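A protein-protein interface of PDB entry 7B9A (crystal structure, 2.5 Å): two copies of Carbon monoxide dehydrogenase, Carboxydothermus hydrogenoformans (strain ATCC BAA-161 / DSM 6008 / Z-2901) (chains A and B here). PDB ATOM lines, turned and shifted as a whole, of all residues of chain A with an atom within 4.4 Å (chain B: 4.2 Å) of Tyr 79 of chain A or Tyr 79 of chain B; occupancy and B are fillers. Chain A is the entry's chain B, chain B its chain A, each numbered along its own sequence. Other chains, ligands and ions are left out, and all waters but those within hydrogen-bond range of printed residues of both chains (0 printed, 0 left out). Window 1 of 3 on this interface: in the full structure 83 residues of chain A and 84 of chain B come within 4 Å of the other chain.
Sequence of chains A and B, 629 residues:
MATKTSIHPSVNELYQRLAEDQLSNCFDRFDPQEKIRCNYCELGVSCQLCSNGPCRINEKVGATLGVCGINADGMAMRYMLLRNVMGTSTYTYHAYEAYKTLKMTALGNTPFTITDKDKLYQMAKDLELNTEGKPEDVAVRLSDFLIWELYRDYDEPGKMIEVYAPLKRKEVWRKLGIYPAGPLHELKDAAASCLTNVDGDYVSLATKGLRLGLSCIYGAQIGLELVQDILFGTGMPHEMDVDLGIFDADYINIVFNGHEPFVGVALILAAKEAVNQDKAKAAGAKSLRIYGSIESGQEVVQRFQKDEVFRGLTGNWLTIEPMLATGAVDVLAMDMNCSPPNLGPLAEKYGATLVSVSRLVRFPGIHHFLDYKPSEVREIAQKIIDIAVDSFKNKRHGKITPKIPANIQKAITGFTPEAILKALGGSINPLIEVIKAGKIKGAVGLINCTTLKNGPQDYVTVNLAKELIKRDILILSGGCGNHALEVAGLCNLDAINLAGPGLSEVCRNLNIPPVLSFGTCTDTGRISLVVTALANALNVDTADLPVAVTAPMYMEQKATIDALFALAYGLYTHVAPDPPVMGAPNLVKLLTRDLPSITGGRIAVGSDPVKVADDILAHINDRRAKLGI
The side-chain amide oxygen of Gln 48 of chain B is in hydrogen-bond range of the side-chain hydroxyl of Tyr 79 of chain A, 2.7 Å away.
The side-chain amide oxygen (OE1) of Gln 48 of chain B sits close to the side-chain amide oxygen (OE1) of Gln 48 of chain A (3.3 Å).
O of Gln 48 of chain B sits at hydrogen-bond distance from NH2 of Arg 83 of chain A (2.8 Å).
The guanidinium group (NH2) of Arg 83 of chain B sits at hydrogen-bond distance from the backbone carbonyl oxygen (O) of Gln 48 of chain A (2.8 Å).
The side-chain hydroxyl of Tyr 79 of chain B sits at hydrogen-bond distance from the side-chain amide oxygen of Gln 48 of chain A (2.6 Å).
OH of Tyr 79 of chain B sits at hydrogen-bond distance from OH of Tyr 79 of chain A (2.9 Å).
The backbone carbonyl oxygen (O) of Tyr 79 of chain B sits close to the guanidinium group (NE) of Arg 83 of chain B (3.4 Å).
Of chain B, only Gln 48 (2.7 Å) and Tyr 79 (2.9 Å) come within 4 Å of Tyr 79 of chain A.
Tyr 79 of chain B touches just these residues of chain A: Gln 48 (2.6 Å) and Tyr 79 (2.9 Å).
Printed residues of chain B within 4 Å of Arg 83 of chain A: Gln 48 (2.8 Å).
Printed residues of chain B within 4 Å of Gln 48 of chain A: Gln 48 (3.3 Å), Tyr 79 (2.6 Å) and Arg 83 (2.8 Å).
Of the printed residues of chain A, Arg 83 of chain B touches Gln 48 (2.8 Å).
Of the printed residues of chain A, Gln 48 of chain B touches Gln 48, Tyr 79 and Arg 83.
The nearest printed residue of chain B that does not touch Tyr 79 of chain A is Leu 82 of chain B (5.1 Å).
The nearest printed residue of chain A that does not touch Tyr 79 of chain B is Leu 82 of chain A (5.4 Å).
Hydrophobic or aromatic side chains of chain B within 4 Å of the printed part of chain A: Tyr 79.
Among the printed residues, no Asp or Glu carboxylate lies within 4 Å of a Lys or Arg side-chain nitrogen of the other chain.
Gln 48 of chain A touches its own counterpart, Gln 48 of chain B.
Gln 48 of chain A touches Tyr 79 of chain B, and with the chains exchanged Tyr 79 of chain A touches Gln 48 of chain B.
Gln 48 of chain A touches Arg 83 of chain B, and with the chains exchanged Arg 83 of chain A touches Gln 48 of chain B.
Tyr 79 of chain A touches its own counterpart, Tyr 79 of chain B.
Positions printed for both chains: 48, 75, 76, 77, 78, 79, 80, 81, 82 and 83.
Of the 6 pairs that touch across the chains among the printed residues, 6 have their exchanged pair printed and touching as well.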
ATOM      1  N   GLN A  48      20.539  -7.648  12.332  1.00  0.00           N
ATOM      2  CA  GLN A  48      19.857  -6.704  13.213  1.00  0.00           C
ATOM      3  C   GLN A  48      19.021  -5.729  12.395  1.00  0.00           C
ATOM      4  O   GLN A  48      18.971  -4.530  12.688  1.00  0.00           O
ATOM      5  CB  GLN A  48      20.852  -5.937  14.089  1.00  0.00           C
ATOM      6  CG  GLN A  48      21.831  -6.800  14.872  1.00  0.00           C
ATOM      7  CD  GLN A  48      23.034  -7.220  14.045  1.00  0.00           C
ATOM      8  OE1 GLN A  48      23.365  -6.586  13.042  1.00  0.00           O
ATOM      9  NE2 GLN A  48      23.692  -8.295  14.460  1.00  0.00           N
ATOM     10  N   MET A  75      21.645 -13.846   4.451  1.00  0.00           N
ATOM     11  CA  MET A  75      21.923 -12.938   5.560  1.00  0.00           C
ATOM     12  C   MET A  75      23.300 -12.292   5.409  1.00  0.00           C
ATOM     13  O   MET A  75      23.432 -11.058   5.430  1.00  0.00           O
ATOM     14  CB  MET A  75      21.814 -13.706   6.881  1.00  0.00           C
ATOM     15  CG  MET A  75      22.128 -12.913   8.140  1.00  0.00           C
ATOM     16  SD  MET A  75      21.909 -13.915   9.630  1.00  0.00           S
ATOM     17  CE  MET A  75      20.156 -14.282   9.547  1.00  0.00           C
ATOM     18  N   ALA A  76      24.336 -13.120   5.241  1.00  0.00           N
ATOM     19  CA  ALA A  76      25.699 -12.605   5.134  1.00  0.00           C
ATOM     20  C   ALA A  76      25.865 -11.721   3.903  1.00  0.00           C
ATOM     21  O   ALA A  76      26.434 -10.624   3.982  1.00  0.00           O
ATOM     22  CB  ALA A  76      26.696 -13.765   5.104  1.00  0.00           C
ATOM     23  N   MET A  77      25.371 -12.180   2.747  1.00  0.00           N
ATOM     24  CA  MET A  77      25.544 -11.392   1.531  1.00  0.00           C
ATOM     25  C   MET A  77      24.771 -10.081   1.594  1.00  0.00           C
ATOM     26  O   MET A  77      25.242  -9.060   1.079  1.00  0.00           O
ATOM     27  CB  MET A  77      25.123 -12.201   0.304  1.00  0.00           C
ATOM     28  CG  MET A  77      25.555 -11.566  -1.004  1.00  0.00           C
ATOM     29  SD  MET A  77      27.327 -11.231  -1.038  1.00  0.00           S
ATOM     30  CE  MET A  77      27.359  -9.651  -1.883  1.00  0.00           C
ATOM     31  N   ARG A  78      23.605 -10.076   2.244  1.00  0.00           N
ATOM     32  CA  ARG A  78      22.836  -8.847   2.375  1.00  0.00           C
ATOM     33  C   ARG A  78      23.543  -7.852   3.281  1.00  0.00           C
ATOM     34  O   ARG A  78      23.580  -6.653   2.981  1.00  0.00           O
ATOM     35  CB  ARG A  78      21.438  -9.164   2.905  1.00  0.00           C
ATOM     36  CG  ARG A  78      20.561  -7.942   3.094  1.00  0.00           C
ATOM     37  CD  ARG A  78      19.151  -8.333   3.496  1.00  0.00           C
ATOM     38  NE  ARG A  78      19.130  -9.105   4.732  1.00  0.00           N
ATOM     39  CZ  ARG A  78      18.020  -9.466   5.366  1.00  0.00           C
ATOM     40  NH1 ARG A  78      16.836  -9.118   4.881  1.00  0.00           N
ATOM     41  NH2 ARG A  78      18.093 -10.169   6.488  1.00  0.00           N
ATOM     42  N   TYR A  79      24.106  -8.321   4.398  1.00  0.00           N
ATOM     43  CA  TYR A  79      24.855  -7.398   5.244  1.00  0.00           C
ATOM     44  C   TYR A  79      26.073  -6.855   4.502  1.00  0.00           C
ATOM     45  O   TYR A  79      26.401  -5.667   4.618  1.00  0.00           O
ATOM     46  CB  TYR A  79      25.267  -8.070   6.556  1.00  0.00           C
ATOM     47  CG  TYR A  79      25.506  -7.084   7.688  1.00  0.00           C
ATOM     48  CD1 TYR A  79      25.459  -5.709   7.467  1.00  0.00           C
ATOM     49  CD2 TYR A  79      25.775  -7.527   8.976  1.00  0.00           C
ATOM     50  CE1 TYR A  79      25.680  -4.807   8.494  1.00  0.00           C
ATOM     51  CE2 TYR A  79      25.995  -6.631  10.010  1.00  0.00           C
ATOM     52  CZ  TYR A  79      25.947  -5.274   9.763  1.00  0.00           C
ATOM     53  OH  TYR A  79      26.166  -4.391  10.794  1.00  0.00           O
ATOM     54  N   MET A  80      26.737  -7.700   3.706  1.00  0.00           N
ATOM     55  CA  MET A  80      27.877  -7.227   2.925  1.00  0.00           C
ATOM     56  C   MET A  80      27.461  -6.157   1.919  1.00  0.00           C
ATOM     57  O   MET A  80      28.150  -5.140   1.763  1.00  0.00           O
ATOM     58  CB  MET A  80      28.550  -8.399   2.211  1.00  0.00           C
ATOM     59  CG  MET A  80      29.514  -7.979   1.111  1.00  0.00           C
ATOM     60  SD  MET A  80      30.485  -9.351   0.460  1.00  0.00           S
ATOM     61  CE  MET A  80      31.621  -9.631   1.815  1.00  0.00           C
ATOM     62  N   LEU A  81      26.341  -6.372   1.223  1.00  0.00           N
ATOM     63  CA  LEU A  81      25.863  -5.389   0.254  1.00  0.00           C
ATOM     64  C   LEU A  81      25.492  -4.076   0.935  1.00  0.00           C
ATOM     65  O   LEU A  81      25.827  -2.988   0.442  1.00  0.00           O
ATOM     66  CB  LEU A  81      24.665  -5.957  -0.508  1.00  0.00           C
ATOM     67  CG  LEU A  81      24.101  -5.139  -1.670  1.00  0.00           C
ATOM     68  CD1 LEU A  81      25.138  -5.001  -2.771  1.00  0.00           C
ATOM     69  CD2 LEU A  81      22.827  -5.775  -2.205  1.00  0.00           C
ATOM     70  N   LEU A  82      24.805  -4.159   2.078  1.00  0.00           N
ATOM     71  CA  LEU A  82      24.442  -2.954   2.815  1.00  0.00           C
ATOM     72  C   LEU A  82      25.680  -2.188   3.263  1.00  0.00           C
ATOM     73  O   LEU A  82      25.703  -0.953   3.217  1.00  0.00           O
ATOM     74  CB  LEU A  82      23.570  -3.317   4.016  1.00  0.00           C
ATOM     75  CG  LEU A  82      23.190  -2.158   4.940  1.00  0.00           C
ATOM     76  CD1 LEU A  82      22.503  -1.051   4.156  1.00  0.00           C
ATOM     77  CD2 LEU A  82      22.302  -2.647   6.072  1.00  0.00           C
ATOM     78  N   ARG A  83      26.720  -2.901   3.699  1.00  0.00           N
ATOM     79  CA  ARG A  83      27.946  -2.222   4.102  1.00  0.00           C
ATOM     80  C   ARG A  83      28.638  -1.569   2.911  1.00  0.00           C
ATOM     81  O   ARG A  83      29.092  -0.422   3.003  1.00  0.00           O
ATOM     82  CB  ARG A  83      28.886  -3.199   4.805  1.00  0.00           C
ATOM     83  CG  ARG A  83      28.560  -3.429   6.273  1.00  0.00           C
ATOM     84  CD  ARG A  83      29.583  -4.344   6.921  1.00  0.00           C
ATOM     85  NE  ARG A  83      29.468  -5.718   6.441  1.00  0.00           N
ATOM     86  CZ  ARG A  83      29.091  -6.742   7.198  1.00  0.00           C
ATOM     87  NH1 ARG A  83      29.009  -7.959   6.680  1.00  0.00           N
ATOM     88  NH2 ARG A  83      28.806  -6.549   8.478  1.00  0.00           N
ATOM     89  N   GLN B  48      29.464  -4.177  13.431  1.00  0.00           N
ATOM     90  CA  GLN B  48      30.015  -5.098  12.441  1.00  0.00           C
ATOM     91  C   GLN B  48      30.495  -4.363  11.192  1.00  0.00           C
ATOM     92  O   GLN B  48      30.503  -4.939  10.098  1.00  0.00           O
ATOM     93  CB  GLN B  48      28.990  -6.158  12.025  1.00  0.00           C
ATOM     94  CG  GLN B  48      28.421  -7.001  13.165  1.00  0.00           C
ATOM     95  CD  GLN B  48      27.242  -6.335  13.857  1.00  0.00           C
ATOM     96  OE1 GLN B  48      26.519  -5.545  13.251  1.00  0.00           O
ATOM     97  NE2 GLN B  48      27.048  -6.650  15.136  1.00  0.00           N
ATOM     98  N   MET B  75      27.796   4.392  18.239  1.00  0.00           N
ATOM     99  CA  MET B  75      27.570   3.083  17.633  1.00  0.00           C
ATOM    100  C   MET B  75      26.091   2.866  17.326  1.00  0.00           C
ATOM    101  O   MET B  75      25.713   2.571  16.181  1.00  0.00           O
ATOM    102  CB  MET B  75      28.104   1.993  18.565  1.00  0.00           C
ATOM    103  CG  MET B  75      27.951   0.572  18.058  1.00  0.00           C
ATOM    104  SD  MET B  75      28.781  -0.607  19.144  1.00  0.00           S
ATOM    105  CE  MET B  75      30.474  -0.028  19.046  1.00  0.00           C
ATOM    106  N   ALA B  76      25.236   3.030  18.340  1.00  0.00           N
ATOM    107  CA  ALA B  76      23.807   2.796  18.155  1.00  0.00           C
ATOM    108  C   ALA B  76      23.218   3.752  17.124  1.00  0.00           C
ATOM    109  O   ALA B  76      22.490   3.332  16.212  1.00  0.00           O
ATOM    110  CB  ALA B  76      23.079   2.927  19.492  1.00  0.00           C
ATOM    111  N   MET B  77      23.525   5.049  17.248  1.00  0.00           N
ATOM    112  CA  MET B  77      22.917   6.020  16.345  1.00  0.00           C
ATOM    113  C   MET B  77      23.405   5.830  14.913  1.00  0.00           C
ATOM    114  O   MET B  77      22.630   5.987  13.960  1.00  0.00           O
ATOM    115  CB  MET B  77      23.197   7.442  16.833  1.00  0.00           C
ATOM    116  CG  MET B  77      22.311   8.489  16.183  1.00  0.00           C
ATOM    117  SD  MET B  77      20.560   8.069  16.289  1.00  0.00           S
ATOM    118  CE  MET B  77      20.047   8.326  14.592  1.00  0.00           C
ATOM    119  N   ARG B  78      24.681   5.470  14.738  1.00  0.00           N
ATOM    120  CA  ARG B  78      25.212   5.237  13.403  1.00  0.00           C
ATOM    121  C   ARG B  78      24.567   4.020  12.760  1.00  0.00           C
ATOM    122  O   ARG B  78      24.234   4.051  11.570  1.00  0.00           O
ATOM    123  CB  ARG B  78      26.730   5.069  13.462  1.00  0.00           C
ATOM    124  CG  ARG B  78      27.367   4.755  12.119  1.00  0.00           C
ATOM    125  CD  ARG B  78      28.875   4.640  12.228  1.00  0.00           C
ATOM    126  NE  ARG B  78      29.282   3.559  13.119  1.00  0.00           N
ATOM    127  CZ  ARG B  78      30.545   3.207  13.334  1.00  0.00           C
ATOM    128  NH1 ARG B  78      31.528   3.851  12.721  1.00  0.00           N
ATOM    129  NH2 ARG B  78      30.828   2.211  14.162  1.00  0.00           N
ATOM    130  N   TYR B  79      24.381   2.936  13.521  1.00  0.00           N
ATOM    131  CA  TYR B  79      23.704   1.771  12.955  1.00  0.00           C
ATOM    132  C   TYR B  79      22.267   2.111  12.566  1.00  0.00           C
ATOM    133  O   TYR B  79      21.786   1.698  11.498  1.00  0.00           O
ATOM    134  CB  TYR B  79      23.739   0.606  13.945  1.00  0.00           C
ATOM    135  CG  TYR B  79      23.628  -0.761  13.300  1.00  0.00           C
ATOM    136  CD1 TYR B  79      23.393  -0.895  11.936  1.00  0.00           C
ATOM    137  CD2 TYR B  79      23.757  -1.919  14.056  1.00  0.00           C
ATOM    138  CE1 TYR B  79      23.290  -2.141  11.346  1.00  0.00           C
ATOM    139  CE2 TYR B  79      23.655  -3.170  13.475  1.00  0.00           C
ATOM    140  CZ  TYR B  79      23.421  -3.274  12.119  1.00  0.00           C
ATOM    141  OH  TYR B  79      23.319  -4.516  11.534  1.00  0.00           O
ATOM    142  N   MET B  80      21.572   2.876  13.416  1.00  0.00           N
ATOM    143  CA  MET B  80      20.205   3.279  13.097  1.00  0.00           C
ATOM    144  C   MET B  80      20.153   4.081  11.800  1.00  0.00           C
ATOM    145  O   MET B  80      19.316   3.818  10.927  1.00  0.00           O
ATOM    146  CB  MET B  80      19.608   4.082  14.253  1.00  0.00           C
ATOM    147  CG  MET B  80      18.292   4.763  13.908  1.00  0.00           C
ATOM    148  SD  MET B  80      17.485   5.528  15.325  1.00  0.00           S
ATOM    149  CE  MET B  80      16.978   4.080  16.249  1.00  0.00           C
ATOM    150  N   LEU B  81      21.041   5.069  11.660  1.00  0.00           N
ATOM    151  CA  LEU B  81      21.076   5.868  10.436  1.00  0.00           C
ATOM    152  C   LEU B  81      21.416   5.008   9.223  1.00  0.00           C
ATOM    153  O   LEU B  81      20.831   5.174   8.141  1.00  0.00           O
ATOM    154  CB  LEU B  81      22.085   7.006  10.592  1.00  0.00           C
ATOM    155  CG  LEU B  81      22.294   7.946   9.405  1.00  0.00           C
ATOM    156  CD1 LEU B  81      21.009   8.685   9.075  1.00  0.00           C
ATOM    157  CD2 LEU B  81      23.423   8.924   9.692  1.00  0.00           C
ATOM    158  N   LEU B  82      22.356   4.073   9.392  1.00  0.00           N
ATOM    159  CA  LEU B  82      22.757   3.202   8.295  1.00  0.00           C
ATOM    160  C   LEU B  82      21.574   2.405   7.766  1.00  0.00           C
ATOM    161  O   LEU B  82      21.374   2.304   6.551  1.00  0.00           O
ATOM    162  CB  LEU B  82      23.875   2.266   8.753  1.00  0.00           C
ATOM    163  CG  LEU B  82      24.236   1.131   7.792  1.00  0.00           C
ATOM    164  CD1 LEU B  82      24.667   1.680   6.440  1.00  0.00           C
ATOM    165  CD2 LEU B  82      25.322   0.249   8.389  1.00  0.00           C
ATOM    166  N   ARG B  83      20.772   1.829   8.662  1.00  0.00           N
ATOM    167  CA  ARG B  83      19.640   1.060   8.154  1.00  0.00           C
ATOM    168  C   ARG B  83      18.466   1.937   7.726  1.00  0.00           C
ATOM    169  O   ARG B  83      17.674   1.505   6.881  1.00  0.00           O
ATOM    170  CB  ARG B  83      19.179   0.008   9.167  1.00  0.00           C
ATOM    171  CG  ARG B  83      19.084   0.461  10.600  1.00  0.00           C
ATOM    172  CD  ARG B  83      19.242  -0.739  11.519  1.00  0.00           C
ATOM    173  NE  ARG B  83      19.477  -0.346  12.903  1.00  0.00           N
ATOM    174  CZ  ARG B  83      20.054  -1.126  13.810  1.00  0.00           C
ATOM    175  NH1 ARG B  83      20.231  -0.686  15.047  1.00  0.00           N
ATOM    176  NH2 ARG B  83      20.465  -2.342  13.479  1.00  0.00           N
